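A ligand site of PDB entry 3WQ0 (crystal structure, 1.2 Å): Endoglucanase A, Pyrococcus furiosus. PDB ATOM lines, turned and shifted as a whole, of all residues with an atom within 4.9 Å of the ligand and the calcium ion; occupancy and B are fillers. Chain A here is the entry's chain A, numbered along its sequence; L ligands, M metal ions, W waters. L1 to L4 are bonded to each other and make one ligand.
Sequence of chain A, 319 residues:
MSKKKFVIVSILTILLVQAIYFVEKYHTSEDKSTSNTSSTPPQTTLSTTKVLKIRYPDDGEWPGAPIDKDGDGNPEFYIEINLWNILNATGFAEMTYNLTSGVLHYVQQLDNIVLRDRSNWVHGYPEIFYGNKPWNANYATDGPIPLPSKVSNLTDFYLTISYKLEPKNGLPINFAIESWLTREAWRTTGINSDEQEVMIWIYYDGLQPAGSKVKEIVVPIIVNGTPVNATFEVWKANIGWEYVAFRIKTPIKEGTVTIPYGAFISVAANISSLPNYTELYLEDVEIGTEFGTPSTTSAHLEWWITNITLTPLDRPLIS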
ATOM      1  N   TRP A  62      16.704  27.075   0.622  1.00  0.00           N
ATOM      2  CA  TRP A  62      15.662  26.219   0.095  1.00  0.00           C
ATOM      3  C   TRP A  62      14.402  27.026  -0.189  1.00  0.00           C
ATOM      4  O   TRP A  62      13.298  26.681   0.255  1.00  0.00           O
ATOM      5  CB  TRP A  62      15.366  25.054   1.069  1.00  0.00           C
ATOM      6  CG  TRP A  62      16.578  24.223   1.340  1.00  0.00           C
ATOM      7  CD1 TRP A  62      17.464  24.359   2.335  1.00  0.00           C
ATOM      8  CD2 TRP A  62      17.044  23.113   0.528  1.00  0.00           C
ATOM      9  NE1 TRP A  62      18.465  23.423   2.265  1.00  0.00           N
ATOM     10  CE2 TRP A  62      18.232  22.618   1.164  1.00  0.00           C
ATOM     11  CE3 TRP A  62      16.529  22.438  -0.614  1.00  0.00           C
ATOM     12  CZ2 TRP A  62      18.925  21.476   0.655  1.00  0.00           C
ATOM     13  CZ3 TRP A  62      17.224  21.347  -1.104  1.00  0.00           C
ATOM     14  CH2 TRP A  62      18.403  20.896  -0.433  1.00  0.00           C
ATOM     15  N   GLU A  80       9.815  25.722  -6.585  1.00  0.00           N
ATOM     16  CA  GLU A  80      10.987  25.581  -5.745  1.00  0.00           C
ATOM     17  C   GLU A  80      12.239  25.958  -6.554  1.00  0.00           C
ATOM     18  O   GLU A  80      12.420  25.457  -7.681  1.00  0.00           O
ATOM     19  CB  GLU A  80      11.207  24.099  -5.279  1.00  0.00           C
ATOM     20  CG  GLU A  80      10.087  23.539  -4.466  1.00  0.00           C
ATOM     21  CD  GLU A  80      10.303  22.126  -3.978  1.00  0.00           C
ATOM     22  OE1 GLU A  80      11.394  21.507  -4.321  1.00  0.00           O
ATOM     23  OE2 GLU A  80       9.407  21.565  -3.309  1.00  0.00           O
ATOM     24  N   ASN A  82      15.187  24.956  -5.534  1.00  0.00           N
ATOM     25  CA  ASN A  82      15.688  23.595  -5.526  1.00  0.00           C
ATOM     26  C   ASN A  82      17.113  23.462  -5.992  1.00  0.00           C
ATOM     27  O   ASN A  82      17.442  22.578  -6.832  1.00  0.00           O
ATOM     28  CB  ASN A  82      14.754  22.662  -6.346  1.00  0.00           C
ATOM     29  CG  ASN A  82      14.990  21.197  -6.085  1.00  0.00           C
ATOM     30  OD1 ASN A  82      15.390  20.822  -4.973  1.00  0.00           O
ATOM     31  ND2 ASN A  82      14.791  20.365  -7.087  1.00  0.00           N
ATOM     32  N   TRP A  84      19.487  21.815  -4.921  1.00  0.00           N
ATOM     33  CA  TRP A  84      19.557  20.809  -3.897  1.00  0.00           C
ATOM     34  C   TRP A  84      20.955  20.266  -3.727  1.00  0.00           C
ATOM     35  O   TRP A  84      21.268  19.760  -2.629  1.00  0.00           O
ATOM     36  CB  TRP A  84      18.530  19.710  -4.144  1.00  0.00           C
ATOM     37  CG  TRP A  84      18.713  18.939  -5.429  1.00  0.00           C
ATOM     38  CD1 TRP A  84      18.121  19.217  -6.646  1.00  0.00           C
ATOM     39  CD2 TRP A  84      19.542  17.790  -5.634  1.00  0.00           C
ATOM     40  NE1 TRP A  84      18.546  18.272  -7.571  1.00  0.00           N
ATOM     41  CE2 TRP A  84      19.401  17.402  -6.970  1.00  0.00           C
ATOM     42  CE3 TRP A  84      20.356  17.032  -4.758  1.00  0.00           C
ATOM     43  CZ2 TRP A  84      20.022  16.232  -7.509  1.00  0.00           C
ATOM     44  CZ3 TRP A  84      20.931  15.833  -5.275  1.00  0.00           C
ATOM     45  CH2 TRP A  84      20.760  15.468  -6.610  1.00  0.00           C
ATOM     46  N   VAL A 122      24.489  16.788 -11.006  1.00  0.00           N
ATOM     47  CA  VAL A 122      23.895  18.077 -11.269  1.00  0.00           C
ATOM     48  C   VAL A 122      23.917  18.932 -10.036  1.00  0.00           C
ATOM     49  O   VAL A 122      24.140  18.501  -8.919  1.00  0.00           O
ATOM     50  CB  VAL A 122      22.440  17.943 -11.818  1.00  0.00           C
ATOM     51  CG1 VAL A 122      22.407  17.189 -13.169  1.00  0.00           C
ATOM     52  CG2 VAL A 122      21.509  17.341 -10.766  1.00  0.00           C
ATOM     53  N   GLY A 124      21.251  21.311  -9.338  1.00  0.00           N
ATOM     54  CA  GLY A 124      19.901  21.635  -8.855  1.00  0.00           C
ATOM     55  C   GLY A 124      18.916  21.421  -9.952  1.00  0.00           C
ATOM     56  O   GLY A 124      19.258  21.067 -11.087  1.00  0.00           O
ATOM     57  N   TYR A 125      17.643  21.673  -9.595  1.00  0.00           N
ATOM     58  CA  TYR A 125      16.505  21.446 -10.521  1.00  0.00           C
ATOM     59  C   TYR A 125      15.412  22.463 -10.147  1.00  0.00           C
ATOM     60  O   TYR A 125      14.373  22.107  -9.579  1.00  0.00           O
ATOM     61  CB  TYR A 125      16.020  19.972 -10.357  1.00  0.00           C
ATOM     62  CG  TYR A 125      14.833  19.539 -11.153  1.00  0.00           C
ATOM     63  CD1 TYR A 125      14.763  19.619 -12.548  1.00  0.00           C
ATOM     64  CD2 TYR A 125      13.722  18.998 -10.500  1.00  0.00           C
ATOM     65  CE1 TYR A 125      13.632  19.187 -13.248  1.00  0.00           C
ATOM     66  CE2 TYR A 125      12.630  18.490 -11.179  1.00  0.00           C
ATOM     67  CZ  TYR A 125      12.555  18.639 -12.552  1.00  0.00           C
ATOM     68  OH  TYR A 125      11.460  18.135 -13.193  1.00  0.00           O
ATOM     69  N   GLU A 127      12.175  24.464 -10.433  1.00  0.00           N
ATOM     70  CA  GLU A 127      11.038  23.713 -10.944  1.00  0.00           C
ATOM     71  C   GLU A 127       9.709  24.278 -10.472  1.00  0.00           C
ATOM     72  O   GLU A 127       9.628  25.047  -9.494  1.00  0.00           O
ATOM     73  CB  GLU A 127      11.107  22.239 -10.495  1.00  0.00           C
ATOM     74  CG  GLU A 127      11.027  22.121  -8.961  1.00  0.00           C
ATOM     75  CD  GLU A 127      10.994  20.663  -8.546  1.00  0.00           C
ATOM     76  OE1 GLU A 127       9.981  20.005  -8.994  1.00  0.00           O
ATOM     77  OE2 GLU A 127      11.858  20.177  -7.874  1.00  0.00           O
ATOM     78  N   ASN A 132       1.984  15.920  -5.173  1.00  0.00           N
ATOM     79  CA  ASN A 132       2.749  15.893  -3.868  1.00  0.00           C
ATOM     80  C   ASN A 132       4.191  15.571  -4.182  1.00  0.00           C
ATOM     81  O   ASN A 132       4.500  14.409  -4.593  1.00  0.00           O
ATOM     82  CB  ASN A 132       2.148  14.838  -2.984  1.00  0.00           C
ATOM     83  CG  ASN A 132       3.030  14.565  -1.830  1.00  0.00           C
ATOM     84  OD1 ASN A 132       3.545  15.513  -1.193  1.00  0.00           O
ATOM     85  ND2 ASN A 132       3.327  13.281  -1.516  1.00  0.00           N
ATOM     86  N   LYS A 133       5.113  16.521  -4.005  1.00  0.00           N
ATOM     87  CA  LYS A 133       6.543  16.156  -4.218  1.00  0.00           C
ATOM     88  C   LYS A 133       6.991  15.332  -2.992  1.00  0.00           C
ATOM     89  O   LYS A 133       6.802  15.767  -1.869  1.00  0.00           O
ATOM     90  CB  LYS A 133       7.379  17.419  -4.364  1.00  0.00           C
ATOM     91  CG  LYS A 133       8.863  17.076  -4.536  1.00  0.00           C
ATOM     92  CD  LYS A 133       9.708  18.238  -5.021  1.00  0.00           C
ATOM     93  CE  LYS A 133      11.183  17.890  -4.929  1.00  0.00           C
ATOM     94  NZ  LYS A 133      12.075  19.044  -5.338  1.00  0.00           N
ATOM     95  N   PRO A 134       7.554  14.133  -3.208  1.00  0.00           N
ATOM     96  CA  PRO A 134       7.713  13.170  -2.076  1.00  0.00           C
ATOM     97  C   PRO A 134       8.923  13.402  -1.238  1.00  0.00           C
ATOM     98  O   PRO A 134       9.160  12.693  -0.274  1.00  0.00           O
ATOM     99  CB  PRO A 134       7.692  11.814  -2.774  1.00  0.00           C
ATOM    100  CG  PRO A 134       8.362  12.124  -4.093  1.00  0.00           C
ATOM    101  CD  PRO A 134       7.734  13.441  -4.528  1.00  0.00           C
ATOM    102  N   TRP A 135       9.742  14.406  -1.586  1.00  0.00           N
ATOM    103  CA  TRP A 135      10.955  14.746  -0.819  1.00  0.00           C
ATOM    104  C   TRP A 135      10.702  15.771   0.279  1.00  0.00           C
ATOM    105  O   TRP A 135      11.641  16.059   1.029  1.00  0.00           O
ATOM    106  CB  TRP A 135      12.044  15.295  -1.816  1.00  0.00           C
ATOM    107  CG  TRP A 135      12.561  14.248  -2.720  1.00  0.00           C
ATOM    108  CD1 TRP A 135      12.165  13.985  -4.010  1.00  0.00           C
ATOM    109  CD2 TRP A 135      13.519  13.258  -2.357  1.00  0.00           C
ATOM    110  NE1 TRP A 135      12.877  12.875  -4.484  1.00  0.00           N
ATOM    111  CE2 TRP A 135      13.690  12.406  -3.493  1.00  0.00           C
ATOM    112  CE3 TRP A 135      14.274  13.029  -1.193  1.00  0.00           C
ATOM    113  CZ2 TRP A 135      14.602  11.295  -3.510  1.00  0.00           C
ATOM    114  CZ3 TRP A 135      15.168  11.918  -1.183  1.00  0.00           C
ATOM    115  CH2 TRP A 135      15.326  11.053  -2.333  1.00  0.00           C
ATOM    116  N   ASN A 136       9.490  16.302   0.343  1.00  0.00           N
ATOM    117  CA  ASN A 136       9.249  17.376   1.356  1.00  0.00           C
ATOM    118  C   ASN A 136       7.762  17.515   1.539  1.00  0.00           C
ATOM    119  O   ASN A 136       6.968  16.719   0.992  1.00  0.00           O
ATOM    120  CB  ASN A 136       9.903  18.688   0.819  1.00  0.00           C
ATOM    121  CG  ASN A 136       9.345  19.118  -0.544  1.00  0.00           C
ATOM    122  OD1 ASN A 136       8.119  19.084  -0.741  1.00  0.00           O
ATOM    123  ND2 ASN A 136      10.218  19.581  -1.435  1.00  0.00           N
ATOM    124  N   ALA A 137       7.346  18.481   2.355  1.00  0.00           N
ATOM    125  CA  ALA A 137       5.947  18.653   2.703  1.00  0.00           C
ATOM    126  C   ALA A 137       5.238  19.636   1.753  1.00  0.00           C
ATOM    127  O   ALA A 137       4.176  20.152   2.139  1.00  0.00           O
ATOM    128  CB  ALA A 137       5.846  19.112   4.172  1.00  0.00           C
ATOM    129  N   ASN A 138       5.762  19.847   0.566  1.00  0.00           N
ATOM    130  CA  ASN A 138       5.136  20.757  -0.359  1.00  0.00           C
ATOM    131  C   ASN A 138       4.235  20.035  -1.304  1.00  0.00           C
ATOM    132  O   ASN A 138       4.551  18.906  -1.772  1.00  0.00           O
ATOM    133  CB  ASN A 138       6.196  21.519  -1.162  1.00  0.00           C
ATOM    134  CG  ASN A 138       7.137  22.287  -0.287  1.00  0.00           C
ATOM    135  OD1 ASN A 138       6.752  22.736   0.830  1.00  0.00           O
ATOM    136  ND2 ASN A 138       8.356  22.525  -0.760  1.00  0.00           N
ATOM    137  N   TYR A 139       3.116  20.655  -1.667  1.00  0.00           N
ATOM    138  CA  TYR A 139       2.108  19.989  -2.510  1.00  0.00           C
ATOM    139  C   TYR A 139       1.267  21.054  -3.242  1.00  0.00           C
ATOM    140  O   TYR A 139       1.192  22.212  -2.810  1.00  0.00           O
ATOM    141  CB  TYR A 139       1.189  19.055  -1.682  1.00  0.00           C
ATOM    142  CG  TYR A 139       0.366  19.851  -0.676  1.00  0.00           C
ATOM    143  CD1 TYR A 139       0.893  20.181   0.585  1.00  0.00           C
ATOM    144  CD2 TYR A 139      -0.907  20.352  -0.993  1.00  0.00           C
ATOM    145  CE1 TYR A 139       0.178  20.978   1.473  1.00  0.00           C
ATOM    146  CE2 TYR A 139      -1.646  21.114  -0.132  1.00  0.00           C
ATOM    147  CZ  TYR A 139      -1.062  21.449   1.079  1.00  0.00           C
ATOM    148  OH  TYR A 139      -1.815  22.236   1.953  1.00  0.00           O
ATOM    149  N   GLU A 178       9.192  15.231 -14.580  1.00  0.00           N
ATOM    150  CA  GLU A 178       9.369  13.974 -13.887  1.00  0.00           C
ATOM    151  C   GLU A 178       8.262  13.701 -12.926  1.00  0.00           C
ATOM    152  O   GLU A 178       7.542  14.582 -12.429  1.00  0.00           O
ATOM    153  CB  GLU A 178      10.696  13.816 -13.229  1.00  0.00           C
ATOM    154  CG  GLU A 178      10.930  14.630 -11.989  1.00  0.00           C
ATOM    155  CD  GLU A 178      12.145  14.131 -11.214  1.00  0.00           C
ATOM    156  OE1 GLU A 178      12.557  12.909 -11.508  1.00  0.00           O
ATOM    157  OE2 GLU A 178      12.817  14.810 -10.441  1.00  0.00           O
ATOM    158  N   TRP A 180       7.500  10.830  -9.494  1.00  0.00           N
ATOM    159  CA  TRP A 180       7.908   9.815  -8.545  1.00  0.00           C
ATOM    160  C   TRP A 180       6.794   8.871  -8.286  1.00  0.00           C
ATOM    161  O   TRP A 180       5.659   9.333  -8.100  1.00  0.00           O
ATOM    162  CB  TRP A 180       8.413  10.510  -7.217  1.00  0.00           C
ATOM    163  CG  TRP A 180       9.521  11.441  -7.411  1.00  0.00           C
ATOM    164  CD1 TRP A 180       9.448  12.758  -7.685  1.00  0.00           C
ATOM    165  CD2 TRP A 180      10.935  11.114  -7.362  1.00  0.00           C
ATOM    166  NE1 TRP A 180      10.705  13.300  -7.803  1.00  0.00           N
ATOM    167  CE2 TRP A 180      11.635  12.297  -7.609  1.00  0.00           C
ATOM    168  CE3 TRP A 180      11.662   9.913  -7.120  1.00  0.00           C
ATOM    169  CZ2 TRP A 180      13.020  12.365  -7.633  1.00  0.00           C
ATOM    170  CZ3 TRP A 180      13.010   9.996  -7.113  1.00  0.00           C
ATOM    171  CH2 TRP A 180      13.717  11.211  -7.344  1.00  0.00           C
ATOM    172  N   ARG A 187       3.689  10.382   0.290  1.00  0.00           N
ATOM    173  CA  ARG A 187       5.034  10.294   0.813  1.00  0.00           C
ATOM    174  C   ARG A 187       5.636  11.664   0.991  1.00  0.00           C
ATOM    175  O   ARG A 187       5.533  12.520   0.040  1.00  0.00           O
ATOM    176  CB  ARG A 187       5.871   9.514  -0.202  1.00  0.00           C
ATOM    177  CG  ARG A 187       7.380   9.485   0.086  1.00  0.00           C
ATOM    178  CD  ARG A 187       7.810   8.709   1.307  1.00  0.00           C
ATOM    179  NE  ARG A 187       7.293   7.350   1.358  1.00  0.00           N
ATOM    180  CZ  ARG A 187       7.717   6.425   0.501  1.00  0.00           C
ATOM    181  NH1 ARG A 187       8.721   6.658  -0.354  1.00  0.00           N
ATOM    182  NH2 ARG A 187       7.118   5.213   0.468  1.00  0.00           N
ATOM    183  N   THR A 188       6.337  11.940   2.069  1.00  0.00           N
ATOM    184  CA  THR A 188       7.011  13.228   2.238  1.00  0.00           C
ATOM    185  C   THR A 188       8.414  13.140   2.748  1.00  0.00           C
ATOM    186  O   THR A 188       9.014  14.182   3.041  1.00  0.00           O
ATOM    187  CB  THR A 188       6.143  14.179   3.124  1.00  0.00           C
ATOM    188  OG1 THR A 188       5.980  13.503   4.405  1.00  0.00           O
ATOM    189  CG2 THR A 188       4.793  14.436   2.524  1.00  0.00           C
ATOM    190  N   GLU A 197      11.563   6.527 -10.211  1.00  0.00           N
ATOM    191  CA  GLU A 197      11.627   7.892 -10.715  1.00  0.00           C
ATOM    192  C   GLU A 197      11.516   7.837 -12.208  1.00  0.00           C
ATOM    193  O   GLU A 197      12.272   7.034 -12.851  1.00  0.00           O
ATOM    194  CB  GLU A 197      12.983   8.497 -10.318  1.00  0.00           C
ATOM    195  CG  GLU A 197      13.121   9.957 -10.741  1.00  0.00           C
ATOM    196  CD  GLU A 197      14.456  10.597 -10.467  1.00  0.00           C
ATOM    197  OE1 GLU A 197      15.408   9.911 -10.023  1.00  0.00           O
ATOM    198  OE2 GLU A 197      14.571  11.829 -10.704  1.00  0.00           O
ATOM    199  N   MET A 199      11.668  10.260 -15.627  1.00  0.00           N
ATOM    200  CA  MET A 199      11.841  11.606 -16.193  1.00  0.00           C
ATOM    201  C   MET A 199      11.697  11.583 -17.683  1.00  0.00           C
ATOM    202  O   MET A 199      12.086  10.617 -18.356  1.00  0.00           O
ATOM    203  CB  MET A 199      13.247  12.106 -15.963  1.00  0.00           C
ATOM    204  CG  MET A 199      13.835  11.811 -14.593  1.00  0.00           C
ATOM    205  SD  MET A 199      15.407  12.715 -14.434  1.00  0.00           S
ATOM    206  CE  MET A 199      14.903  14.349 -13.914  1.00  0.00           C
ATOM    207  N   ILE A 239      19.708   3.674  -8.714  1.00  0.00           N
ATOM    208  CA  ILE A 239      20.445   4.784  -8.052  1.00  0.00           C
ATOM    209  C   ILE A 239      19.929   4.992  -6.623  1.00  0.00           C
ATOM    210  O   ILE A 239      20.027   6.110  -6.074  1.00  0.00           O
ATOM    211  CB  ILE A 239      20.349   6.087  -8.875  1.00  0.00           C
ATOM    212  CG1 ILE A 239      18.881   6.535  -9.111  1.00  0.00           C
ATOM    213  CG2 ILE A 239      21.063   5.863 -10.211  1.00  0.00           C
ATOM    214  CD1 ILE A 239      18.795   7.918  -9.689  1.00  0.00           C
ATOM    215  N   TRP A 241      16.896   3.714  -6.065  1.00  0.00           N
ATOM    216  CA  TRP A 241      15.520   3.442  -6.528  1.00  0.00           C
ATOM    217  C   TRP A 241      15.702   3.172  -8.027  1.00  0.00           C
ATOM    218  O   TRP A 241      16.805   3.389  -8.592  1.00  0.00           O
ATOM    219  CB  TRP A 241      14.569   4.661  -6.275  1.00  0.00           C
ATOM    220  CG  TRP A 241      15.098   5.965  -6.807  1.00  0.00           C
ATOM    221  CD1 TRP A 241      14.951   6.466  -8.073  1.00  0.00           C
ATOM    222  CD2 TRP A 241      15.807   6.944  -6.050  1.00  0.00           C
ATOM    223  NE1 TRP A 241      15.560   7.707  -8.134  1.00  0.00           N
ATOM    224  CE2 TRP A 241      16.087   8.021  -6.904  1.00  0.00           C
ATOM    225  CE3 TRP A 241      16.243   7.034  -4.661  1.00  0.00           C
ATOM    226  CZ2 TRP A 241      16.756   9.150  -6.488  1.00  0.00           C
ATOM    227  CZ3 TRP A 241      16.898   8.188  -4.232  1.00  0.00           C
ATOM    228  CH2 TRP A 241      17.136   9.228  -5.139  1.00  0.00           C
ATOM    229  N   TYR A 243      15.293   4.068 -11.815  1.00  0.00           N
ATOM    230  CA  TYR A 243      15.228   5.297 -12.572  1.00  0.00           C
ATOM    231  C   TYR A 243      14.980   4.966 -14.003  1.00  0.00           C
ATOM    232  O   TYR A 243      15.729   4.108 -14.584  1.00  0.00           O
ATOM    233  CB  TYR A 243      16.548   5.999 -12.383  1.00  0.00           C
ATOM    234  CG  TYR A 243      16.891   7.156 -13.281  1.00  0.00           C
ATOM    235  CD1 TYR A 243      17.408   6.973 -14.540  1.00  0.00           C
ATOM    236  CD2 TYR A 243      16.678   8.467 -12.819  1.00  0.00           C
ATOM    237  CE1 TYR A 243      17.789   8.047 -15.308  1.00  0.00           C
ATOM    238  CE2 TYR A 243      17.080   9.563 -13.554  1.00  0.00           C
ATOM    239  CZ  TYR A 243      17.649   9.334 -14.821  1.00  0.00           C
ATOM    240  OH  TYR A 243      18.131  10.355 -15.595  1.00  0.00           O
ATOM    241  N   GLU A 286       6.490  17.105 -12.103  1.00  0.00           N
ATOM    242  CA  GLU A 286       7.423  18.199 -11.879  1.00  0.00           C
ATOM    243  C   GLU A 286       7.978  18.665 -13.201  1.00  0.00           C
ATOM    244  O   GLU A 286       8.203  17.819 -14.080  1.00  0.00           O
ATOM    245  CB  GLU A 286       8.565  17.750 -10.960  1.00  0.00           C
ATOM    246  CG  GLU A 286       8.091  17.102  -9.665  1.00  0.00           C
ATOM    247  CD  GLU A 286       9.165  16.799  -8.673  1.00  0.00           C
ATOM    248  OE1 GLU A 286      10.203  17.494  -8.590  1.00  0.00           O
ATOM    249  OE2 GLU A 286       9.034  15.794  -7.910  1.00  0.00           O
ATOM    250  N   GLU A 290      17.207  20.765 -14.851  1.00  0.00           N
ATOM    251  CA  GLU A 290      18.401  20.330 -14.116  1.00  0.00           C
ATOM    252  C   GLU A 290      19.592  20.972 -14.843  1.00  0.00           C
ATOM    253  O   GLU A 290      19.589  21.150 -16.062  1.00  0.00           O
ATOM    254  CB  GLU A 290      18.544  18.807 -14.131  1.00  0.00           C
HETATM  255  C1  LIG L   1      17.782  12.551  -9.601  1.00  0.00           C
HETATM  256  C2  LIG L   1      16.785  13.012  -8.566  1.00  0.00           C
HETATM  257  C3  LIG L   1      16.734  14.559  -8.583  1.00  0.00           C
HETATM  258  C4  LIG L   1      16.381  15.008  -9.997  1.00  0.00           C
HETATM  259  C5  LIG L   1      16.365  16.472 -10.218  1.00  0.00           C
HETATM  260  C6  LIG L   1      17.446  13.014 -11.061  1.00  0.00           C
HETATM  261  O1  LIG L   1      18.371  12.761 -12.017  1.00  0.00           O
HETATM  262  O2  LIG L   1      17.842  11.118  -9.611  1.00  0.00           O
HETATM  263  O3  LIG L   1      17.182  12.552  -7.264  1.00  0.00           O
HETATM  264  O4  LIG L   1      15.642  15.020  -7.730  1.00  0.00           O
HETATM  265  O5  LIG L   1      17.422  14.525 -10.877  1.00  0.00           O
HETATM  266  O6  LIG L   1      17.653  17.064 -10.004  1.00  0.00           O
HETATM  267  C1  LG2 L   2      14.886  16.403  -5.904  1.00  0.00           C
HETATM  268  C2  LG2 L   2      15.387  17.010  -4.634  1.00  0.00           C
HETATM  269  C3  LG2 L   2      16.003  16.000  -3.703  1.00  0.00           C
HETATM  270  C4  LG2 L   2      17.040  15.151  -4.434  1.00  0.00           C
HETATM  271  C5  LG2 L   2      17.384  13.882  -3.605  1.00  0.00           C
HETATM  272  C6  LG2 L   2      16.069  15.639  -6.551  1.00  0.00           C
HETATM  273  O1  LG2 L   2      14.419  17.416  -6.767  1.00  0.00           O
HETATM  274  O2  LG2 L   2      14.274  17.645  -3.979  1.00  0.00           O
HETATM  275  O3  LG2 L   2      16.751  16.605  -2.662  1.00  0.00           O
HETATM  276  O4  LG2 L   2      16.452  14.604  -5.650  1.00  0.00           O
HETATM  277  O5  LG2 L   2      18.634  13.360  -3.975  1.00  0.00           O
HETATM  278  C1  LG3 L   3      17.222  16.703  -0.349  1.00  0.00           C
HETATM  279  C2  LG3 L   3      16.643  16.974   1.026  1.00  0.00           C
HETATM  280  C3  LG3 L   3      15.838  18.315   0.946  1.00  0.00           C
HETATM  281  C4  LG3 L   3      14.775  18.168  -0.127  1.00  0.00           C
HETATM  282  C5  LG3 L   3      13.981  19.460  -0.280  1.00  0.00           C
HETATM  283  C6  LG3 L   3      16.132  16.712  -1.395  1.00  0.00           C
HETATM  284  O1  LG3 L   3      17.796  15.378  -0.296  1.00  0.00           O
HETATM  285  O2  LG3 L   3      17.698  17.133   1.950  1.00  0.00           O
HETATM  286  O3  LG3 L   3      15.171  18.459   2.220  1.00  0.00           O
HETATM  287  O4  LG3 L   3      15.438  17.936  -1.387  1.00  0.00           O
HETATM  288  O5  LG3 L   3      13.051  19.331  -1.337  1.00  0.00           O
HETATM  289  C1  LG4 L   4      14.299  19.980   3.888  1.00  0.00           C
HETATM  290  C2  LG4 L   4      14.530  21.274   4.657  1.00  0.00           C
HETATM  291  C3  LG4 L   4      15.920  21.197   5.200  1.00  0.00           C
HETATM  292  C4  LG4 L   4      16.917  20.987   4.058  1.00  0.00           C
HETATM  293  C5  LG4 L   4      18.330  20.999   4.560  1.00  0.00           C
HETATM  294  C6  LG4 L   4      15.349  19.765   2.813  1.00  0.00           C
HETATM  295  O1  LG4 L   4      13.014  19.996   3.265  1.00  0.00           O
HETATM  296  O2  LG4 L   4      13.562  21.285   5.709  1.00  0.00           O
HETATM  297  O3  LG4 L   4      16.188  22.498   5.737  1.00  0.00           O
HETATM  298  O4  LG4 L   4      16.609  19.717   3.446  1.00  0.00           O
HETATM  299  O5  LG4 L   4      18.457  19.879   5.481  1.00  0.00           O
HETATM  300 CA    CA M   1       5.292  16.975  -0.613  1.00  0.00          CA
HETATM  301  O   HOH W   1      13.651  21.360  -2.981  1.00  0.00           O
HETATM  302  O   HOH W   2      17.887  13.548   1.591  1.00  0.00           O
HETATM  303  O   HOH W   3      20.080  14.985  -1.799  1.00  0.00           O
HETATM  304  O   HOH W   4      20.268  10.816 -11.079  1.00  0.00           O
HETATM  305  O   HOH W   5      17.285  17.205   4.724  1.00  0.00           O
HETATM  306  O   HOH W   6       3.416  17.390   0.831  1.00  0.00           O
HETATM  307  O   HOH W   7      20.317  18.195   1.463  1.00  0.00           O
HETATM  308  O   HOH W   8      12.151  17.509   3.323  1.00  0.00           O
HETATM  309  O   HOH W   9      12.460  16.097  -8.043  1.00  0.00           O
HETATM  310  O   HOH W  10      15.527  25.195   5.236  1.00  0.00           O
HETATM  311  O   HOH W  11      19.063  15.930 -12.416  1.00  0.00           O
HETATM  312  O   HOH W  12      19.706  11.759  -6.458  1.00  0.00           O
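The indole nitrogen (NE1) of Trp 84 sits at hydrogen-bond distance from an oxygen (O6) of LIG L1, 2.9 Å away. The side-chain amide nitrogen (ND2) of Asn 136 lies within hydrogen-bond range of an oxygen (O5) of LG3 L3 (2.8 Å). An oxygen (O2) of LG2 L2 lies within hydrogen-bond range of the side-chain amino group (NZ) of Lys 133 (2.9 Å). OE1 of Glu 197 sits at hydrogen-bond distance from O2 of LIG L1 (2.7 Å). ND2 of Asn 82 sits at hydrogen-bond distance from O1 of LG2 L2, at 3.0 Å.
The backbone NH (N) of Glu 286 is in hydrogen-bond range of the backbone carbonyl oxygen (O) of Glu 178, 2.8 Å away. The side-chain hydroxyl (OH) of Tyr 125 lies within hydrogen-bond range of the backbone carbonyl oxygen (O) of Glu 286, at 3.4 Å. The indole nitrogen (NE1) of Trp 180 sits at hydrogen-bond distance from the side-chain carboxylate (OE2) of Glu 286. N of Asn 138 sits at hydrogen-bond distance from OD1 of Asn 136, at 2.8 Å. The side-chain amide nitrogen (ND2) of Asn 82 is in hydrogen-bond range of the side-chain carboxylate (OE2) of Glu 127 (3.0 Å). The side-chain sulfur of Met 199 sits close to the side-chain hydroxyl of Tyr 243. ND2 of Asn 136 lies within hydrogen-bond range of OE2 of Glu 80 (2.8 Å). The backbone carbonyl oxygen of Thr 188 sits at hydrogen-bond distance from the backbone NH of Asn 136 (3.5 Å).
Residues that only touch the ligand: Trp 62, Val 122, Tyr 125, Glu 127, Trp 135, Glu 178, Trp 180, Met 199, Ile 239, Trp 241 and Tyr 243. Hydrophobic or aromatic side chains within 4 Å of the ligand: Trp 62, Trp 84, Val 122, Tyr 125, Trp 135, Trp 180, Met 199, Ile 239, Trp 241 and Tyr 243. Of the 27 residues printed, 16 come within 4 Å of the ligand. The nearest printed residue that does not touch the ligand is Glu 80 (4.05 Å).
Ala 137 touches the calcium ion.
O of Lys 133 is bound to the calcium ion (2.3 Å). O of Asn 136 binds the calcium ion (2.3 Å). The calcium ion is bound by the side-chain amide oxygen (OD1) of Asn 132 (2.4 Å). The backbone carbonyl oxygen (O) of Asn 138 is bound to the calcium ion, 2.4 Å away. Water W6 binds the calcium ion. The calcium ion has five donor atoms within binding distance. Slightly farther from the calcium ion lies the backbone nitrogen (N) of Asn 138 (3.1 Å).
Water W8 lies within hydrogen-bond range of an oxygen (O1) of LG4 L4 (2.6 Å) and the backbone carbonyl oxygen (O) of Trp 135 (2.8 Å). Water W1 lies within hydrogen-bond range of OE1 of Glu 80, O5 of LG3 L3 and OD1 of Asn 82. Water W9 lies within hydrogen-bond range of O1 of LG2 L2, OE1 of Glu 286, OE2 of Glu 178 and NE1 of Trp 180.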
